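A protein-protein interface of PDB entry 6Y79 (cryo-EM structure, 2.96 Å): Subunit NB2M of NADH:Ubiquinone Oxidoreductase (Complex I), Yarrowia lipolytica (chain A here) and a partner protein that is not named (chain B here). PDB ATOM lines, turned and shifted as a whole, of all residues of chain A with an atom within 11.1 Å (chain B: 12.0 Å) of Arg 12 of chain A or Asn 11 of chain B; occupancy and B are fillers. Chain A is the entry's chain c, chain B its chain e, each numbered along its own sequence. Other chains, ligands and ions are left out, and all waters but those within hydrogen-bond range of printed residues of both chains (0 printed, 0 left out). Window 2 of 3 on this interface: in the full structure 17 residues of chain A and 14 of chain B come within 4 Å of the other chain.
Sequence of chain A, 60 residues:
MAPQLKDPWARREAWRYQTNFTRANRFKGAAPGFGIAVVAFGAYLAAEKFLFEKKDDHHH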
ATOM      1  N   ASP A   7      25.593  -1.058 -26.025  1.00  0.00           N
ATOM      2  CA  ASP A   7      24.142  -1.024 -25.882  1.00  0.00           C
ATOM      3  C   ASP A   7      23.692   0.408 -25.644  1.00  0.00           C
ATOM      4  O   ASP A   7      24.110   1.023 -24.650  1.00  0.00           O
ATOM      5  CB  ASP A   7      23.690  -1.923 -24.731  1.00  0.00           C
ATOM      6  CG  ASP A   7      22.193  -2.198 -24.752  1.00  0.00           C
ATOM      7  OD1 ASP A   7      21.401  -1.276 -24.467  1.00  0.00           O
ATOM      8  OD2 ASP A   7      21.803  -3.343 -25.048  1.00  0.00           O
ATOM      9  N   PRO A   8      22.850   0.981 -26.509  1.00  0.00           N
ATOM     10  CA  PRO A   8      22.435   2.373 -26.298  1.00  0.00           C
ATOM     11  C   PRO A   8      21.504   2.575 -25.121  1.00  0.00           C
ATOM     12  O   PRO A   8      21.528   3.644 -24.514  1.00  0.00           O
ATOM     13  CB  PRO A   8      21.744   2.740 -27.617  1.00  0.00           C
ATOM     14  CG  PRO A   8      22.343   1.833 -28.607  1.00  0.00           C
ATOM     15  CD  PRO A   8      22.558   0.542 -27.880  1.00  0.00           C
ATOM     16  N   TRP A   9      20.672   1.608 -24.763  1.00  0.00           N
ATOM     17  CA  TRP A   9      19.855   1.723 -23.553  1.00  0.00           C
ATOM     18  C   TRP A   9      20.542   0.913 -22.457  1.00  0.00           C
ATOM     19  O   TRP A   9      20.052  -0.118 -21.998  1.00  0.00           O
ATOM     20  CB  TRP A   9      18.421   1.263 -23.808  1.00  0.00           C
ATOM     21  CG  TRP A   9      17.626   2.233 -24.656  1.00  0.00           C
ATOM     22  CD1 TRP A   9      17.388   2.144 -25.990  1.00  0.00           C
ATOM     23  CD2 TRP A   9      16.956   3.421 -24.216  1.00  0.00           C
ATOM     24  NE1 TRP A   9      16.618   3.191 -26.414  1.00  0.00           N
ATOM     25  CE2 TRP A   9      16.332   3.989 -25.340  1.00  0.00           C
ATOM     26  CE3 TRP A   9      16.825   4.058 -22.985  1.00  0.00           C
ATOM     27  CZ2 TRP A   9      15.597   5.168 -25.269  1.00  0.00           C
ATOM     28  CZ3 TRP A   9      16.089   5.218 -22.913  1.00  0.00           C
ATOM     29  CH2 TRP A   9      15.483   5.762 -24.046  1.00  0.00           C
ATOM     30  N   ALA A  10      21.694   1.408 -22.020  1.00  0.00           N
ATOM     31  CA  ALA A  10      22.440   0.757 -20.953  1.00  0.00           C
ATOM     32  C   ALA A  10      22.154   1.348 -19.586  1.00  0.00           C
ATOM     33  O   ALA A  10      22.198   0.621 -18.586  1.00  0.00           O
ATOM     34  CB  ALA A  10      23.948   0.839 -21.221  1.00  0.00           C
ATOM     35  N   ARG A  11      21.870   2.648 -19.516  1.00  0.00           N
ATOM     36  CA  ARG A  11      21.558   3.274 -18.244  1.00  0.00           C
ATOM     37  C   ARG A  11      20.087   3.168 -17.893  1.00  0.00           C
ATOM     38  O   ARG A  11      19.733   3.350 -16.722  1.00  0.00           O
ATOM     39  CB  ARG A  11      21.977   4.746 -18.266  1.00  0.00           C
ATOM     40  CG  ARG A  11      23.483   4.978 -18.342  1.00  0.00           C
ATOM     41  CD  ARG A  11      23.800   6.464 -18.438  1.00  0.00           C
ATOM     42  NE  ARG A  11      23.481   7.023 -19.751  1.00  0.00           N
ATOM     43  CZ  ARG A  11      23.427   8.325 -20.019  1.00  0.00           C
ATOM     44  NH1 ARG A  11      23.131   8.740 -21.240  1.00  0.00           N
ATOM     45  NH2 ARG A  11      23.665   9.216 -19.064  1.00  0.00           N
ATOM     46  N   ARG A  12      19.226   2.894 -18.877  1.00  0.00           N
ATOM     47  CA  ARG A  12      17.840   2.567 -18.569  1.00  0.00           C
ATOM     48  C   ARG A  12      17.740   1.234 -17.850  1.00  0.00           C
ATOM     49  O   ARG A  12      17.218   1.159 -16.737  1.00  0.00           O
ATOM     50  CB  ARG A  12      16.986   2.520 -19.829  1.00  0.00           C
ATOM     51  CG  ARG A  12      15.543   2.149 -19.498  1.00  0.00           C
ATOM     52  CD  ARG A  12      14.574   2.202 -20.667  1.00  0.00           C
ATOM     53  NE  ARG A  12      13.210   2.125 -20.155  1.00  0.00           N
ATOM     54  CZ  ARG A  12      12.121   1.988 -20.900  1.00  0.00           C
ATOM     55  NH1 ARG A  12      12.221   1.883 -22.212  1.00  0.00           N
ATOM     56  NH2 ARG A  12      10.926   1.934 -20.325  1.00  0.00           N
ATOM     57  N   GLU A  13      18.245   0.173 -18.465  1.00  0.00           N
ATOM     58  CA  GLU A  13      18.058  -1.180 -17.948  1.00  0.00           C
ATOM     59  C   GLU A  13      19.155  -1.586 -16.981  1.00  0.00           C
ATOM     60  O   GLU A  13      19.811  -2.609 -17.147  1.00  0.00           O
ATOM     61  CB  GLU A  13      17.978  -2.151 -19.105  1.00  0.00           C
ATOM     62  CG  GLU A  13      16.947  -1.757 -20.101  1.00  0.00           C
ATOM     63  CD  GLU A  13      17.025  -2.614 -21.306  1.00  0.00           C
ATOM     64  OE1 GLU A  13      18.123  -3.160 -21.526  1.00  0.00           O
ATOM     65  OE2 GLU A  13      16.002  -2.742 -22.005  1.00  0.00           O
ATOM     66  N   ALA A  14      19.363  -0.771 -15.957  1.00  0.00           N
ATOM     67  CA  ALA A  14      20.215  -1.158 -14.850  1.00  0.00           C
ATOM     68  C   ALA A  14      19.420  -1.533 -13.615  1.00  0.00           C
ATOM     69  O   ALA A  14      19.884  -2.356 -12.822  1.00  0.00           O
ATOM     70  CB  ALA A  14      21.188  -0.029 -14.504  1.00  0.00           C
ATOM     71  N   TRP A  15      18.219  -0.971 -13.455  1.00  0.00           N
ATOM     72  CA  TRP A  15      17.420  -1.220 -12.263  1.00  0.00           C
ATOM     73  C   TRP A  15      16.847  -2.623 -12.222  1.00  0.00           C
ATOM     74  O   TRP A  15      16.442  -3.079 -11.150  1.00  0.00           O
ATOM     75  CB  TRP A  15      16.284  -0.209 -12.164  1.00  0.00           C
ATOM     76  CG  TRP A  15      15.305  -0.240 -13.293  1.00  0.00           C
ATOM     77  CD1 TRP A  15      15.384   0.456 -14.448  1.00  0.00           C
ATOM     78  CD2 TRP A  15      14.081  -0.977 -13.353  1.00  0.00           C
ATOM     79  NE1 TRP A  15      14.301   0.192 -15.242  1.00  0.00           N
ATOM     80  CE2 TRP A  15      13.482  -0.687 -14.588  1.00  0.00           C
ATOM     81  CE3 TRP A  15      13.438  -1.863 -12.485  1.00  0.00           C
ATOM     82  CZ2 TRP A  15      12.271  -1.245 -14.978  1.00  0.00           C
ATOM     83  CZ3 TRP A  15      12.237  -2.413 -12.871  1.00  0.00           C
ATOM     84  CH2 TRP A  15      11.666  -2.106 -14.106  1.00  0.00           C
ATOM     85  N   ARG A  16      16.798  -3.313 -13.359  1.00  0.00           N
ATOM     86  CA  ARG A  16      16.325  -4.688 -13.380  1.00  0.00           C
ATOM     87  C   ARG A  16      17.351  -5.662 -12.823  1.00  0.00           C
ATOM     88  O   ARG A  16      17.005  -6.811 -12.540  1.00  0.00           O
ATOM     89  CB  ARG A  16      15.955  -5.082 -14.803  1.00  0.00           C
ATOM     90  CG  ARG A  16      14.874  -4.231 -15.397  1.00  0.00           C
ATOM     91  CD  ARG A  16      14.611  -4.616 -16.825  1.00  0.00           C
ATOM     92  NE  ARG A  16      13.322  -4.104 -17.267  1.00  0.00           N
ATOM     93  CZ  ARG A  16      13.152  -2.931 -17.859  1.00  0.00           C
ATOM     94  NH1 ARG A  16      11.942  -2.544 -18.223  1.00  0.00           N
ATOM     95  NH2 ARG A  16      14.197  -2.151 -18.092  1.00  0.00           N
ATOM     96  N   TYR A  17      18.602  -5.239 -12.679  1.00  0.00           N
ATOM     97  CA  TYR A  17      19.661  -6.095 -12.170  1.00  0.00           C
ATOM     98  C   TYR A  17      20.196  -5.635 -10.829  1.00  0.00           C
ATOM     99  O   TYR A  17      21.003  -6.343 -10.222  1.00  0.00           O
ATOM    100  CB  TYR A  17      20.802  -6.167 -13.189  1.00  0.00           C
ATOM    101  CG  TYR A  17      20.367  -6.862 -14.442  1.00  0.00           C
ATOM    102  CD1 TYR A  17      20.382  -8.243 -14.517  1.00  0.00           C
ATOM    103  CD2 TYR A  17      19.896  -6.145 -15.538  1.00  0.00           C
ATOM    104  CE1 TYR A  17      19.970  -8.897 -15.649  1.00  0.00           C
ATOM    105  CE2 TYR A  17      19.476  -6.790 -16.678  1.00  0.00           C
ATOM    106  CZ  TYR A  17      19.519  -8.169 -16.725  1.00  0.00           C
ATOM    107  OH  TYR A  17      19.105  -8.842 -17.841  1.00  0.00           O
ATOM    108  N   GLN A  18      19.763  -4.478 -10.360  1.00  0.00           N
ATOM    109  CA  GLN A  18      20.227  -3.880  -9.122  1.00  0.00           C
ATOM    110  C   GLN A  18      19.310  -4.313  -7.976  1.00  0.00           C
ATOM    111  O   GLN A  18      18.590  -5.309  -8.084  1.00  0.00           O
ATOM    112  CB  GLN A  18      20.362  -2.366  -9.303  1.00  0.00           C
ATOM    113  CG  GLN A  18      21.621  -2.004 -10.081  1.00  0.00           C
ATOM    114  CD  GLN A  18      21.649  -0.575 -10.567  1.00  0.00           C
ATOM    115  OE1 GLN A  18      20.771   0.220 -10.247  1.00  0.00           O
ATOM    116  NE2 GLN A  18      22.663  -0.241 -11.359  1.00  0.00           N
ATOM    117  N   THR A  19      19.320  -3.539  -6.892  1.00  0.00           N
ATOM    118  CA  THR A  19      19.108  -3.897  -5.490  1.00  0.00           C
ATOM    119  C   THR A  19      18.072  -4.966  -5.120  1.00  0.00           C
ATOM    120  O   THR A  19      18.292  -5.704  -4.156  1.00  0.00           O
ATOM    121  CB  THR A  19      18.784  -2.599  -4.754  1.00  0.00           C
ATOM    122  OG1 THR A  19      18.441  -2.861  -3.391  1.00  0.00           O
ATOM    123  CG2 THR A  19      17.691  -1.849  -5.466  1.00  0.00           C
ATOM    124  N   ASN B   7       7.010   7.024  -5.868  1.00  0.00           N
ATOM    125  CA  ASN B   7       7.314   7.224  -7.278  1.00  0.00           C
ATOM    126  C   ASN B   7       8.685   7.844  -7.482  1.00  0.00           C
ATOM    127  O   ASN B   7       9.100   8.031  -8.616  1.00  0.00           O
ATOM    128  CB  ASN B   7       6.273   8.133  -7.944  1.00  0.00           C
ATOM    129  CG  ASN B   7       4.855   7.811  -7.527  1.00  0.00           C
ATOM    130  OD1 ASN B   7       4.185   6.992  -8.155  1.00  0.00           O
ATOM    131  ND2 ASN B   7       4.376   8.477  -6.481  1.00  0.00           N
ATOM    132  N   TYR B   8       9.396   8.099  -6.379  1.00  0.00           N
ATOM    133  CA  TYR B   8      10.360   9.199  -6.312  1.00  0.00           C
ATOM    134  C   TYR B   8      11.563   9.034  -7.235  1.00  0.00           C
ATOM    135  O   TYR B   8      12.184  10.037  -7.603  1.00  0.00           O
ATOM    136  CB  TYR B   8      10.843   9.383  -4.872  1.00  0.00           C
ATOM    137  CG  TYR B   8       9.772   9.857  -3.908  1.00  0.00           C
ATOM    138  CD1 TYR B   8       8.598  10.453  -4.368  1.00  0.00           C
ATOM    139  CD2 TYR B   8       9.935   9.708  -2.538  1.00  0.00           C
ATOM    140  CE1 TYR B   8       7.621  10.878  -3.495  1.00  0.00           C
ATOM    141  CE2 TYR B   8       8.964  10.134  -1.654  1.00  0.00           C
ATOM    142  CZ  TYR B   8       7.808  10.718  -2.139  1.00  0.00           C
ATOM    143  OH  TYR B   8       6.833  11.144  -1.264  1.00  0.00           O
ATOM    144  N   LYS B   9      11.900   7.813  -7.632  1.00  0.00           N
ATOM    145  CA  LYS B   9      12.956   7.592  -8.604  1.00  0.00           C
ATOM    146  C   LYS B   9      12.366   7.052  -9.898  1.00  0.00           C
ATOM    147  O   LYS B   9      11.291   6.447  -9.904  1.00  0.00           O
ATOM    148  CB  LYS B   9      14.002   6.610  -8.082  1.00  0.00           C
ATOM    149  CG  LYS B   9      14.659   7.012  -6.788  1.00  0.00           C
ATOM    150  CD  LYS B   9      15.636   5.942  -6.361  1.00  0.00           C
ATOM    151  CE  LYS B   9      16.410   6.333  -5.119  1.00  0.00           C
ATOM    152  NZ  LYS B   9      17.346   5.252  -4.699  1.00  0.00           N
ATOM    153  N   TRP B  10      13.074   7.280 -10.996  1.00  0.00           N
ATOM    154  CA  TRP B  10      12.741   6.648 -12.258  1.00  0.00           C
ATOM    155  C   TRP B  10      13.994   6.085 -12.902  1.00  0.00           C
ATOM    156  O   TRP B  10      15.058   6.716 -12.890  1.00  0.00           O
ATOM    157  CB  TRP B  10      12.044   7.623 -13.208  1.00  0.00           C
ATOM    158  CG  TRP B  10      10.652   7.886 -12.778  1.00  0.00           C
ATOM    159  CD1 TRP B  10       9.548   7.144 -13.075  1.00  0.00           C
ATOM    160  CD2 TRP B  10      10.206   8.952 -11.942  1.00  0.00           C
ATOM    161  NE1 TRP B  10       8.441   7.680 -12.471  1.00  0.00           N
ATOM    162  CE2 TRP B  10       8.817   8.801 -11.780  1.00  0.00           C
ATOM    163  CE3 TRP B  10      10.846  10.023 -11.320  1.00  0.00           C
ATOM    164  CZ2 TRP B  10       8.054   9.689 -11.029  1.00  0.00           C
ATOM    165  CZ3 TRP B  10      10.093  10.895 -10.567  1.00  0.00           C
ATOM    166  CH2 TRP B  10       8.712  10.719 -10.421  1.00  0.00           C
ATOM    167  N   ASN B  11      13.819   4.880 -13.463  1.00  0.00           N
ATOM    168  CA  ASN B  11      14.815   4.064 -14.156  1.00  0.00           C
ATOM    169  C   ASN B  11      16.152   4.028 -13.425  1.00  0.00           C
ATOM    170  O   ASN B  11      17.221   4.173 -14.024  1.00  0.00           O
ATOM    171  CB  ASN B  11      14.951   4.552 -15.598  1.00  0.00           C
ATOM    172  CG  ASN B  11      13.689   4.294 -16.400  1.00  0.00           C
ATOM    173  OD1 ASN B  11      12.645   3.986 -15.823  1.00  0.00           O
ATOM    174  ND2 ASN B  11      13.774   4.407 -17.723  1.00  0.00           N
ATOM    175  N   GLY B  12      16.070   3.841 -12.114  1.00  0.00           N
ATOM    176  CA  GLY B  12      17.206   3.661 -11.247  1.00  0.00           C
ATOM    177  C   GLY B  12      16.759   2.749 -10.130  1.00  0.00           C
ATOM    178  O   GLY B  12      15.636   2.237 -10.163  1.00  0.00           O
ATOM    179  N   PRO B  13      17.601   2.560  -9.110  1.00  0.00           N
ATOM    180  CA  PRO B  13      17.390   1.469  -8.142  1.00  0.00           C
ATOM    181  C   PRO B  13      16.134   1.645  -7.299  1.00  0.00           C
ATOM    182  O   PRO B  13      15.899   2.701  -6.710  1.00  0.00           O
ATOM    183  CB  PRO B  13      18.652   1.521  -7.272  1.00  0.00           C
ATOM    184  CG  PRO B  13      19.621   2.374  -8.015  1.00  0.00           C
ATOM    185  CD  PRO B  13      18.813   3.336  -8.808  1.00  0.00           C
ATOM    186  N   LEU B  14      15.326   0.591  -7.251  1.00  0.00           N
ATOM    187  CA  LEU B  14      14.065   0.612  -6.534  1.00  0.00           C
ATOM    188  C   LEU B  14      14.330   0.561  -5.028  1.00  0.00           C
ATOM    189  O   LEU B  14      15.439   0.250  -4.598  1.00  0.00           O
ATOM    190  CB  LEU B  14      13.201  -0.569  -6.974  1.00  0.00           C
ATOM    191  CG  LEU B  14      12.251  -0.496  -8.184  1.00  0.00           C
ATOM    192  CD1 LEU B  14      11.047   0.368  -7.889  1.00  0.00           C
ATOM    193  CD2 LEU B  14      12.934  -0.025  -9.461  1.00  0.00           C
ATOM    194  N   PRO B  15      13.357   0.918  -4.202  1.00  0.00           N
ATOM    195  CA  PRO B  15      13.501   0.651  -2.769  1.00  0.00           C
ATOM    196  C   PRO B  15      13.099  -0.774  -2.422  1.00  0.00           C
ATOM    197  O   PRO B  15      12.423  -1.468  -3.184  1.00  0.00           O
ATOM    198  CB  PRO B  15      12.558   1.665  -2.118  1.00  0.00           C
ATOM    199  CG  PRO B  15      11.557   1.960  -3.164  1.00  0.00           C
ATOM    200  CD  PRO B  15      12.289   1.898  -4.464  1.00  0.00           C
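Hydrophobic or aromatic side chains of chain B within 4 Å of the printed part of chain A: Pro 13 and Leu 14.
Of chain B, only Asn 11 comes within 4 Å of Arg 12 of chain A. Of the printed residues of chain A, Asn 11 of chain B touches Arg 11, Arg 12 and Trp 15. No residue of chain B comes within 4 Å of Trp 9 of chain A. No residue of chain B comes within 4 Å of Ala 14 of chain A. Of chain B, only Asn 11, Gly 12 and Leu 14 come within 4 Å of Trp 15 of chain A. Gly 12 of chain B touches just one residue of chain A: Trp 15. Printed residues of chain A within 4 Å of Leu 14 of chain B: Trp 15 (3.6 Å) and Thr 19 (3.2 Å). Of the printed residues of chain B, Thr 19 of chain A touches Pro 13 and Leu 14. Printed residues of chain A within 4 Å of Pro 13 of chain B: Gln 18 and Thr 19. Printed residues of chain B within 4 Å of Gln 18 of chain A: Pro 13 (3.3 Å). Pro 15 of chain B touches none of the printed residues of chain A.
The backbone carbonyl oxygen of Arg 12 of chain A lies close to the indole nitrogen of Trp 15 of chain A (3.4 Å).
ND2 of Asn 11 of chain B lies close to NE of Arg 12 of chain A, at 3.4 Å.
Asn 11 of chain B touches Arg 11 of chain A (O to O, 3.8 Å). CD1 of Trp 15 of chain A touches CA of Asn 11 of chain B, 3.7 Å away. CB of Trp 15 of chain A touches O of Gly 12 of chain B (3.2 Å). Trp 15 of chain A touches Leu 14 of chain B (CE3 to CD2, 3.6 Å). Gln 18 of chain A touches Pro 13 of chain B (OE1 to CG, 3.3 Å). Thr 19 of chain A touches Pro 13 of chain B. CG2 of Thr 19 of chain A touches O of Leu 14 of chain B, 3.2 Å away.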
